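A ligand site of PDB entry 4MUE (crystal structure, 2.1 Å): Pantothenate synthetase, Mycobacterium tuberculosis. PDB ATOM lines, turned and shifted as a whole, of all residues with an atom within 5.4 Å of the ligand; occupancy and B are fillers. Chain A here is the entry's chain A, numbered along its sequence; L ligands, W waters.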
ATOM      1  N   PRO A  38       0.303 -23.827 -10.504  1.00  0.00           N
ATOM      2  CA  PRO A  38      -0.535 -22.841  -9.780  1.00  0.00           C
ATOM      3  C   PRO A  38      -0.184 -22.850  -8.307  1.00  0.00           C
ATOM      4  O   PRO A  38      -0.127 -23.933  -7.688  1.00  0.00           O
ATOM      5  CB  PRO A  38      -1.975 -23.377  -9.956  1.00  0.00           C
ATOM      6  CG  PRO A  38      -1.923 -24.372 -11.045  1.00  0.00           C
ATOM      7  CD  PRO A  38      -0.503 -24.925 -11.098  1.00  0.00           C
ATOM      8  N   THR A  39       0.064 -21.679  -7.732  1.00  0.00           N
ATOM      9  CA  THR A  39       0.393 -21.669  -6.324  1.00  0.00           C
ATOM     10  C   THR A  39      -0.358 -20.567  -5.549  1.00  0.00           C
ATOM     11  O   THR A  39      -0.923 -19.652  -6.135  1.00  0.00           O
ATOM     12  CB  THR A  39       1.936 -21.551  -6.041  1.00  0.00           C
ATOM     13  OG1 THR A  39       2.337 -20.159  -6.041  1.00  0.00           O
ATOM     14  CG2 THR A  39       2.796 -22.418  -6.989  1.00  0.00           C
ATOM     15  N   MET A  40      -0.321 -20.688  -4.225  1.00  0.00           N
ATOM     16  CA  MET A  40      -0.771 -19.615  -3.342  1.00  0.00           C
ATOM     17  C   MET A  40       0.397 -18.912  -2.752  1.00  0.00           C
ATOM     18  O   MET A  40       0.277 -18.322  -1.690  1.00  0.00           O
ATOM     19  CB  MET A  40      -1.595 -20.170  -2.202  1.00  0.00           C
ATOM     20  CG  MET A  40      -2.845 -20.745  -2.678  1.00  0.00           C
ATOM     21  SD  MET A  40      -4.017 -21.088  -1.355  1.00  0.00           S
ATOM     22  CE  MET A  40      -3.482 -22.616  -0.656  1.00  0.00           C
ATOM     23  N   GLY A  41       1.528 -18.971  -3.423  1.00  0.00           N
ATOM     24  CA  GLY A  41       2.756 -18.385  -2.914  1.00  0.00           C
ATOM     25  C   GLY A  41       3.231 -19.128  -1.652  1.00  0.00           C
ATOM     26  O   GLY A  41       2.837 -20.308  -1.408  1.00  0.00           O
ATOM     27  N   HIS A  44       7.753 -23.466  -1.137  1.00  0.00           N
ATOM     28  CA  HIS A  44       8.752 -24.296  -0.516  1.00  0.00           C
ATOM     29  C   HIS A  44       9.299 -25.307  -1.531  1.00  0.00           C
ATOM     30  O   HIS A  44       8.950 -25.308  -2.765  1.00  0.00           O
ATOM     31  CB  HIS A  44       8.089 -24.986   0.661  1.00  0.00           C
ATOM     32  CG  HIS A  44       6.817 -25.696   0.291  1.00  0.00           C
ATOM     33  ND1 HIS A  44       6.806 -26.847  -0.477  1.00  0.00           N
ATOM     34  CD2 HIS A  44       5.526 -25.422   0.581  1.00  0.00           C
ATOM     35  CE1 HIS A  44       5.554 -27.255  -0.631  1.00  0.00           C
ATOM     36  NE2 HIS A  44       4.760 -26.410   0.000  1.00  0.00           N
ATOM     37  N   GLY A  46       8.576 -28.292  -2.154  1.00  0.00           N
ATOM     38  CA  GLY A  46       7.611 -29.110  -2.921  1.00  0.00           C
ATOM     39  C   GLY A  46       7.221 -28.378  -4.224  1.00  0.00           C
ATOM     40  O   GLY A  46       7.111 -28.985  -5.275  1.00  0.00           O
ATOM     41  N   HIS A  47       7.039 -27.061  -4.124  1.00  0.00           N
ATOM     42  CA  HIS A  47       6.808 -26.238  -5.304  1.00  0.00           C
ATOM     43  C   HIS A  47       8.004 -26.271  -6.256  1.00  0.00           C
ATOM     44  O   HIS A  47       7.815 -26.294  -7.468  1.00  0.00           O
ATOM     45  CB  HIS A  47       6.487 -24.772  -4.942  1.00  0.00           C
ATOM     46  CG  HIS A  47       5.306 -24.633  -4.052  1.00  0.00           C
ATOM     47  ND1 HIS A  47       5.412 -24.252  -2.725  1.00  0.00           N
ATOM     48  CD2 HIS A  47       3.984 -24.846  -4.281  1.00  0.00           C
ATOM     49  CE1 HIS A  47       4.204 -24.234  -2.186  1.00  0.00           C
ATOM     50  NE2 HIS A  47       3.326 -24.600  -3.109  1.00  0.00           N
ATOM     51  N   ALA A  49      10.072 -28.681  -6.601  1.00  0.00           N
ATOM     52  CA  ALA A  49       9.848 -29.955  -7.304  1.00  0.00           C
ATOM     53  C   ALA A  49       8.786 -29.891  -8.441  1.00  0.00           C
ATOM     54  O   ALA A  49       8.900 -30.626  -9.422  1.00  0.00           O
ATOM     55  CB  ALA A  49       9.473 -31.082  -6.327  1.00  0.00           C
ATOM     56  N   LEU A  50       7.732 -29.074  -8.284  1.00  0.00           N
ATOM     57  CA  LEU A  50       6.716 -28.957  -9.356  1.00  0.00           C
ATOM     58  C   LEU A  50       7.357 -28.227 -10.503  1.00  0.00           C
ATOM     59  O   LEU A  50       7.144 -28.591 -11.647  1.00  0.00           O
ATOM     60  CB  LEU A  50       5.484 -28.165  -8.897  1.00  0.00           C
ATOM     61  CG  LEU A  50       4.629 -28.728  -7.714  1.00  0.00           C
ATOM     62  CD1 LEU A  50       3.276 -27.992  -7.530  1.00  0.00           C
ATOM     63  CD2 LEU A  50       4.393 -30.179  -7.945  1.00  0.00           C
ATOM     64  N   TYR A  82      -3.437 -16.002   6.582  1.00  0.00           N
ATOM     65  CA  TYR A  82      -2.787 -16.791   5.555  1.00  0.00           C
ATOM     66  C   TYR A  82      -1.364 -16.271   5.209  1.00  0.00           C
ATOM     67  O   TYR A  82      -1.187 -15.049   5.092  1.00  0.00           O
ATOM     68  CB  TYR A  82      -3.661 -16.892   4.285  1.00  0.00           C
ATOM     69  CG  TYR A  82      -3.224 -18.098   3.523  1.00  0.00           C
ATOM     70  CD1 TYR A  82      -3.774 -19.348   3.792  1.00  0.00           C
ATOM     71  CD2 TYR A  82      -2.174 -18.009   2.596  1.00  0.00           C
ATOM     72  CE1 TYR A  82      -3.327 -20.490   3.133  1.00  0.00           C
ATOM     73  CE2 TYR A  82      -1.714 -19.135   1.940  1.00  0.00           C
ATOM     74  CZ  TYR A  82      -2.294 -20.372   2.207  1.00  0.00           C
ATOM     75  OH  TYR A  82      -1.842 -21.496   1.570  1.00  0.00           O
ATOM     76  N   VAL A 139     -12.085 -23.424  -5.161  1.00  0.00           N
ATOM     77  CA  VAL A 139     -10.834 -23.987  -5.773  1.00  0.00           C
ATOM     78  C   VAL A 139     -11.014 -24.290  -7.301  1.00  0.00           C
ATOM     79  O   VAL A 139     -10.221 -23.854  -8.113  1.00  0.00           O
ATOM     80  CB  VAL A 139     -10.385 -25.260  -5.033  1.00  0.00           C
ATOM     81  CG1 VAL A 139      -9.151 -25.885  -5.729  1.00  0.00           C
ATOM     82  CG2 VAL A 139     -10.007 -24.914  -3.575  1.00  0.00           C
ATOM     83  N   VAL A 142     -11.348 -21.040  -9.393  1.00  0.00           N
ATOM     84  CA  VAL A 142     -10.101 -20.285  -9.675  1.00  0.00           C
ATOM     85  C   VAL A 142      -9.160 -21.068 -10.592  1.00  0.00           C
ATOM     86  O   VAL A 142      -8.514 -20.498 -11.500  1.00  0.00           O
ATOM     87  CB  VAL A 142      -9.390 -19.737  -8.398  1.00  0.00           C
ATOM     88  CG1 VAL A 142      -8.767 -20.881  -7.522  1.00  0.00           C
ATOM     89  CG2 VAL A 142      -8.311 -18.680  -8.795  1.00  0.00           C
ATOM     90  N   VAL A 143      -9.119 -22.385 -10.412  1.00  0.00           N
ATOM     91  CA  VAL A 143      -8.238 -23.223 -11.259  1.00  0.00           C
ATOM     92  C   VAL A 143      -8.708 -23.170 -12.707  1.00  0.00           C
ATOM     93  O   VAL A 143      -7.876 -23.031 -13.605  1.00  0.00           O
ATOM     94  CB  VAL A 143      -8.165 -24.658 -10.759  1.00  0.00           C
ATOM     95  CG1 VAL A 143      -7.498 -25.611 -11.780  1.00  0.00           C
ATOM     96  CG2 VAL A 143      -7.341 -24.729  -9.485  1.00  0.00           C
ATOM     97  N   LEU A 146      -7.563 -19.891 -14.066  1.00  0.00           N
ATOM     98  CA  LEU A 146      -6.119 -19.892 -14.366  1.00  0.00           C
ATOM     99  C   LEU A 146      -5.841 -20.714 -15.628  1.00  0.00           C
ATOM    100  O   LEU A 146      -5.033 -20.287 -16.456  1.00  0.00           O
ATOM    101  CB  LEU A 146      -5.283 -20.463 -13.194  1.00  0.00           C
ATOM    102  CG  LEU A 146      -5.290 -19.539 -11.950  1.00  0.00           C
ATOM    103  CD1 LEU A 146      -4.728 -20.285 -10.719  1.00  0.00           C
ATOM    104  CD2 LEU A 146      -4.537 -18.197 -12.154  1.00  0.00           C
ATOM    105  N   PHE A 157       0.472 -30.394  -9.943  1.00  0.00           N
ATOM    106  CA  PHE A 157       0.060 -30.323  -8.567  1.00  0.00           C
ATOM    107  C   PHE A 157       0.840 -31.374  -7.762  1.00  0.00           C
ATOM    108  O   PHE A 157       1.143 -32.471  -8.288  1.00  0.00           O
ATOM    109  CB  PHE A 157      -1.434 -30.590  -8.444  1.00  0.00           C
ATOM    110  CG  PHE A 157      -2.307 -29.585  -9.213  1.00  0.00           C
ATOM    111  CD1 PHE A 157      -2.566 -28.334  -8.713  1.00  0.00           C
ATOM    112  CD2 PHE A 157      -2.847 -29.921 -10.421  1.00  0.00           C
ATOM    113  CE1 PHE A 157      -3.345 -27.425  -9.412  1.00  0.00           C
ATOM    114  CE2 PHE A 157      -3.651 -29.056 -11.124  1.00  0.00           C
ATOM    115  CZ  PHE A 157      -3.887 -27.784 -10.629  1.00  0.00           C
ATOM    116  N   GLY A 158       1.098 -31.048  -6.488  1.00  0.00           N
ATOM    117  CA  GLY A 158       1.596 -32.024  -5.510  1.00  0.00           C
ATOM    118  C   GLY A 158       0.468 -32.968  -5.125  1.00  0.00           C
ATOM    119  O   GLY A 158      -0.700 -32.593  -5.146  1.00  0.00           O
ATOM    120  N   GLU A 159       0.796 -34.205  -4.716  1.00  0.00           N
ATOM    121  CA  GLU A 159      -0.238 -35.187  -4.354  1.00  0.00           C
ATOM    122  C   GLU A 159      -0.725 -35.056  -2.950  1.00  0.00           C
ATOM    123  O   GLU A 159      -1.655 -35.782  -2.508  1.00  0.00           O
ATOM    124  CB  GLU A 159       0.239 -36.592  -4.557  1.00  0.00           C
ATOM    125  CG  GLU A 159       0.518 -36.880  -6.084  1.00  0.00           C
ATOM    126  CD  GLU A 159       1.019 -38.330  -6.303  1.00  0.00           C
ATOM    127  OE1 GLU A 159       1.254 -39.018  -5.281  1.00  0.00           O
ATOM    128  OE2 GLU A 159       1.207 -38.745  -7.460  1.00  0.00           O
ATOM    129  N   LYS A 160      -0.077 -34.175  -2.195  1.00  0.00           N
ATOM    130  CA  LYS A 160      -0.437 -34.076  -0.781  1.00  0.00           C
ATOM    131  C   LYS A 160      -1.945 -33.719  -0.639  1.00  0.00           C
ATOM    132  O   LYS A 160      -2.674 -34.342   0.158  1.00  0.00           O
ATOM    133  CB  LYS A 160       0.458 -33.053  -0.069  1.00  0.00           C
ATOM    134  CG  LYS A 160       0.346 -33.144   1.487  1.00  0.00           C
ATOM    135  CD  LYS A 160      -0.682 -32.226   2.104  1.00  0.00           C
ATOM    136  CE  LYS A 160      -0.028 -31.024   2.701  1.00  0.00           C
ATOM    137  NZ  LYS A 160      -0.935 -29.817   2.614  1.00  0.00           N
ATOM    138  N   ASP A 161      -2.417 -32.728  -1.404  1.00  0.00           N
ATOM    139  CA  ASP A 161      -3.825 -32.397  -1.361  1.00  0.00           C
ATOM    140  C   ASP A 161      -4.515 -33.244  -2.374  1.00  0.00           C
ATOM    141  O   ASP A 161      -4.775 -32.817  -3.523  1.00  0.00           O
ATOM    142  CB  ASP A 161      -4.041 -30.906  -1.652  1.00  0.00           C
ATOM    143  CG  ASP A 161      -3.433 -30.029  -0.566  1.00  0.00           C
ATOM    144  OD1 ASP A 161      -3.998 -30.005   0.498  1.00  0.00           O
ATOM    145  OD2 ASP A 161      -2.358 -29.410  -0.767  1.00  0.00           O
ATOM    146  N   GLN A 164      -8.311 -32.663  -3.600  1.00  0.00           N
ATOM    147  CA  GLN A 164      -8.265 -31.509  -4.491  1.00  0.00           C
ATOM    148  C   GLN A 164      -7.740 -31.864  -5.872  1.00  0.00           C
ATOM    149  O   GLN A 164      -8.290 -31.411  -6.897  1.00  0.00           O
ATOM    150  CB  GLN A 164      -7.478 -30.335  -3.861  1.00  0.00           C
ATOM    151  CG  GLN A 164      -7.042 -29.288  -4.902  1.00  0.00           C
ATOM    152  CD  GLN A 164      -6.068 -28.286  -4.297  1.00  0.00           C
ATOM    153  OE1 GLN A 164      -6.428 -27.551  -3.389  1.00  0.00           O
ATOM    154  NE2 GLN A 164      -4.821 -28.281  -4.781  1.00  0.00           N
ATOM    155  N   ILE A 168      -9.806 -31.778  -9.477  1.00  0.00           N
ATOM    156  CA  ILE A 168      -9.233 -31.146 -10.648  1.00  0.00           C
ATOM    157  C   ILE A 168      -9.230 -32.027 -11.889  1.00  0.00           C
ATOM    158  O   ILE A 168      -9.609 -31.582 -12.945  1.00  0.00           O
ATOM    159  CB  ILE A 168      -7.868 -30.502 -10.352  1.00  0.00           C
ATOM    160  CG1 ILE A 168      -8.079 -29.378  -9.288  1.00  0.00           C
ATOM    161  CG2 ILE A 168      -7.259 -29.991 -11.677  1.00  0.00           C
ATOM    162  CD1 ILE A 168      -6.749 -28.715  -8.599  1.00  0.00           C
ATOM    163  N   VAL A 184       2.523 -34.839  -8.804  1.00  0.00           N
ATOM    164  CA  VAL A 184       3.901 -35.082  -8.418  1.00  0.00           C
ATOM    165  C   VAL A 184       4.006 -35.541  -6.969  1.00  0.00           C
ATOM    166  O   VAL A 184       3.415 -34.907  -6.092  1.00  0.00           O
ATOM    167  CB  VAL A 184       4.644 -33.818  -8.519  1.00  0.00           C
ATOM    168  CG1 VAL A 184       6.201 -33.985  -8.020  1.00  0.00           C
ATOM    169  CG2 VAL A 184       4.527 -33.318  -9.924  1.00  0.00           C
ATOM    170  N   PRO A 185       4.760 -36.639  -6.696  1.00  0.00           N
ATOM    171  CA  PRO A 185       4.830 -37.122  -5.311  1.00  0.00           C
ATOM    172  C   PRO A 185       5.238 -36.054  -4.315  1.00  0.00           C
ATOM    173  O   PRO A 185       6.067 -35.198  -4.631  1.00  0.00           O
ATOM    174  CB  PRO A 185       5.889 -38.251  -5.403  1.00  0.00           C
ATOM    175  CG  PRO A 185       5.454 -38.932  -6.686  1.00  0.00           C
ATOM    176  CD  PRO A 185       5.385 -37.632  -7.598  1.00  0.00           C
ATOM    177  N   THR A 186       4.603 -36.109  -3.148  1.00  0.00           N
ATOM    178  CA  THR A 186       4.799 -35.140  -2.070  1.00  0.00           C
ATOM    179  C   THR A 186       6.240 -35.165  -1.570  1.00  0.00           C
ATOM    180  O   THR A 186       6.743 -36.186  -1.123  1.00  0.00           O
ATOM    181  CB  THR A 186       3.838 -35.535  -0.939  1.00  0.00           C
ATOM    182  OG1 THR A 186       2.522 -35.556  -1.482  1.00  0.00           O
ATOM    183  CG2 THR A 186       3.929 -34.607   0.267  1.00  0.00           C
ATOM    184  N   VAL A 187       6.920 -34.039  -1.719  1.00  0.00           N
ATOM    185  CA  VAL A 187       8.201 -33.810  -1.120  1.00  0.00           C
ATOM    186  C   VAL A 187       8.024 -33.803   0.429  1.00  0.00           C
ATOM    187  O   VAL A 187       7.045 -33.238   0.919  1.00  0.00           O
ATOM    188  CB  VAL A 187       8.794 -32.444  -1.691  1.00  0.00           C
ATOM    189  CG1 VAL A 187      10.045 -32.045  -0.942  1.00  0.00           C
ATOM    190  CG2 VAL A 187       9.082 -32.571  -3.192  1.00  0.00           C
ATOM    191  N   MET A 195       5.591 -31.820   3.173  1.00  0.00           N
ATOM    192  CA  MET A 195       5.840 -30.367   3.064  1.00  0.00           C
ATOM    193  C   MET A 195       4.534 -29.606   3.057  1.00  0.00           C
ATOM    194  O   MET A 195       3.537 -30.011   2.439  1.00  0.00           O
ATOM    195  CB  MET A 195       6.576 -30.037   1.759  1.00  0.00           C
ATOM    196  CG  MET A 195       8.041 -30.439   1.757  1.00  0.00           C
ATOM    197  SD  MET A 195       9.190 -29.234   2.467  1.00  0.00           S
ATOM    198  CE  MET A 195      10.789 -30.062   2.206  1.00  0.00           C
ATOM    199  N   SER A 196       4.550 -28.469   3.732  1.00  0.00           N
ATOM    200  CA  SER A 196       3.391 -27.601   3.756  1.00  0.00           C
ATOM    201  C   SER A 196       3.790 -26.260   4.301  1.00  0.00           C
ATOM    202  O   SER A 196       4.594 -26.175   5.212  1.00  0.00           O
ATOM    203  CB  SER A 196       2.285 -28.158   4.659  1.00  0.00           C
ATOM    204  OG  SER A 196       1.215 -27.229   4.655  1.00  0.00           O
ATOM    205  N   SER A 197       3.174 -25.243   3.693  1.00  0.00           N
ATOM    206  CA  SER A 197       3.223 -23.859   4.132  1.00  0.00           C
ATOM    207  C   SER A 197       2.853 -23.789   5.599  1.00  0.00           C
ATOM    208  O   SER A 197       3.500 -23.088   6.389  1.00  0.00           O
ATOM    209  CB  SER A 197       2.218 -23.022   3.302  1.00  0.00           C
ATOM    210  OG  SER A 197       0.877 -23.323   3.671  1.00  0.00           O
ATOM    211  N   ARG A 198       1.825 -24.563   5.967  1.00  0.00           N
ATOM    212  CA  ARG A 198       1.244 -24.509   7.292  1.00  0.00           C
ATOM    213  C   ARG A 198       2.040 -25.199   8.432  1.00  0.00           C
ATOM    214  O   ARG A 198       1.613 -25.180   9.593  1.00  0.00           O
ATOM    215  CB  ARG A 198      -0.213 -24.967   7.271  1.00  0.00           C
ATOM    216  CG  ARG A 198      -1.140 -23.964   6.546  1.00  0.00           C
ATOM    217  CD  ARG A 198      -2.448 -23.847   7.293  1.00  0.00           C
ATOM    218  NE  ARG A 198      -3.110 -25.161   7.431  1.00  0.00           N
ATOM    219  CZ  ARG A 198      -4.394 -25.396   7.144  1.00  0.00           C
ATOM    220  NH1 ARG A 198      -4.904 -26.614   7.284  1.00  0.00           N
ATOM    221  NH2 ARG A 198      -5.179 -24.413   6.713  1.00  0.00           N
HETATM  222  O1  LIG L   1       0.357 -27.524   1.940  1.00  0.00           O
HETATM  223  C1  LIG L   1       1.129 -27.369   1.016  1.00  0.00           C
HETATM  224  O2  LIG L   1       1.950 -26.413   0.846  1.00  0.00           O
HETATM  225  C2  LIG L   1       1.184 -28.569   0.140  1.00  0.00           C
HETATM  226  N1  LIG L   1       1.730 -28.474  -1.239  1.00  0.00           N
HETATM  227  C3  LIG L   1       2.685 -29.359  -1.566  1.00  0.00           C
HETATM  228  C4  LIG L   1       3.266 -30.298  -0.798  1.00  0.00           C
HETATM  229  C5  LIG L   1       4.235 -31.136  -1.352  1.00  0.00           C
HETATM  230  C6  LIG L   1       4.607 -30.953  -2.690  1.00  0.00           C
HETATM  231  O3  LIG L   1       5.544 -31.808  -3.157  1.00  0.00           O
HETATM  232  C7  LIG L   1       5.550 -31.847  -4.606  1.00  0.00           C
HETATM  233  C8  LIG L   1       3.961 -29.940  -3.482  1.00  0.00           C
HETATM  234  C9  LIG L   1       3.016 -29.158  -2.879  1.00  0.00           C
HETATM  235  C10 LIG L   1       2.253 -28.127  -3.318  1.00  0.00           C
HETATM  236  C11 LIG L   1       1.441 -27.715  -2.313  1.00  0.00           C
HETATM  237  C12 LIG L   1       0.509 -26.712  -2.274  1.00  0.00           C
HETATM  238  O4  LIG L   1      -0.512 -26.834  -1.580  1.00  0.00           O
HETATM  239  N2  LIG L   1       0.759 -25.575  -2.956  1.00  0.00           N
HETATM  240  S1  LIG L   1      -0.182 -24.323  -2.717  1.00  0.00           S
HETATM  241  O5  LIG L   1      -1.145 -24.248  -1.649  1.00  0.00           O
HETATM  242  O6  LIG L   1       0.389 -22.994  -3.139  1.00  0.00           O
HETATM  243  C13 LIG L   1      -1.534 -24.668  -3.834  1.00  0.00           C
HETATM  244  C14 LIG L   1      -1.366 -24.878  -5.198  1.00  0.00           C
HETATM  245  C15 LIG L   1      -2.527 -25.052  -5.986  1.00  0.00           C
HETATM  246  C16 LIG L   1      -3.848 -25.053  -5.465  1.00  0.00           C
HETATM  247  C17 LIG L   1      -4.965 -25.163  -6.363  1.00  0.00           C
HETATM  248  F1  LIG L   1      -6.064 -24.518  -5.951  1.00  0.00           F
HETATM  249  F2  LIG L   1      -4.578 -24.426  -7.521  1.00  0.00           F
HETATM  250  F3  LIG L   1      -5.303 -26.363  -6.731  1.00  0.00           F
HETATM  251  C18 LIG L   1      -3.985 -24.857  -4.098  1.00  0.00           C
HETATM  252  C19 LIG L   1      -2.828 -24.667  -3.304  1.00  0.00           C
HETATM  253  O   HOH W   1       1.906 -22.612  -0.302  1.00  0.00           O
HETATM  254  O   HOH W   2      -0.070 -28.289  -5.759  1.00  0.00           O
HETATM  255  O   HOH W   3      -1.360 -25.067   3.081  1.00  0.00           O
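The backbone NH (N) of Met 40 is in hydrogen-bond range of an oxygen (O6) of the ligand, 2.6 Å away.
An oxygen (O1) of the ligand lies within salt-bridge range of the side-chain amino group (NZ) of Lys 160.
A ring nitrogen (NE2) of His 47 sits at hydrogen-bond distance from a nitrogen (N2) of the ligand (2.8 Å).
O1 of the ligand is in hydrogen-bond range of OG of Ser 196.
O2 of the ligand sits at hydrogen-bond distance from NE2 of His 44, 2.9 Å away.
The backbone NH (N) of Val 187 is in hydrogen-bond range of an oxygen (O3) of the ligand, 3.0 Å away.
An oxygen (O2) of the ligand is in hydrogen-bond range of the backbone NH of Ser 197, at 3.3 Å.
SD of Met 40 lies close to OH of Tyr 82 (3.7 Å).
The side-chain amino group (NZ) of Lys 160 is in salt-bridge range of the side-chain carboxylate (OD2) of Asp 161 (3.7 Å).
The side-chain hydroxyl (OG1) of Thr 186 sits at hydrogen-bond distance from the backbone NH (N) of Lys 160 (3.0 Å).
The side-chain hydroxyl (OG) of Ser 196 is in hydrogen-bond range of the backbone NH (N) of Arg 198.
The backbone NH (N) of Gly 46 is in hydrogen-bond range of a ring nitrogen (ND1) of His 44.
The backbone carbonyl oxygen of Val 187 sits at hydrogen-bond distance from the backbone NH of Met 195.
The backbone NH (N) of Gly 41 lies within hydrogen-bond range of the side-chain hydroxyl (OG1) of Thr 39 (3.0 Å).
The backbone carbonyl oxygen (O) of Phe 157 sits at hydrogen-bond distance from the backbone NH (N) of Val 184 (2.8 Å).
The side-chain carboxylate (OD2) of Asp 161 lies close to an oxygen (O4) of the ligand (3.3 Å).
The side-chain amide nitrogen of Gln 164 sits close to a fluorine (F3) of the ligand.
Pro 38 touches the ligand.
Thr 39 touches the ligand (CA to O6, 3.4 Å).
Gly 46 touches the ligand.
CD2 of Leu 50 touches C7 of the ligand, at 3.9 Å.
Val 139 touches the ligand (CG1 to F1, 3.4 Å).
Val 143 touches the ligand (CG2 to F2, 3.4 Å).
Phe 157 touches the ligand.
CA of Gly 158 touches C8 of the ligand (3.7 Å).
CD1 of Ile 168 touches F3 of the ligand, 3.3 Å away.
O of Pro 185 touches C7 of the ligand, at 3.4 Å.
CA of Thr 186 touches O3 of the ligand, at 3.6 Å.
Met 195 touches the ligand.
Hydrophobic or aromatic side chains within 4 Å of the ligand: Pro 38, Met 40, His 44, His 47, Leu 50, Val 139, Val 143, Phe 157, Ile 168 and Val 187.
Along chain A the residues within 4 Å of the ligand span positions 38 to 197.
The nearest printed residue that does not touch the ligand is Val 184 (4.02 Å).
Water W3 lies within hydrogen-bond range of OG of Ser 197 (2.9 Å) and O1 of the ligand (3.2 Å).
Water W1 lies within hydrogen-bond range of O of Gly 41 (2.7 Å) and O6 of the ligand (3.2 Å).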
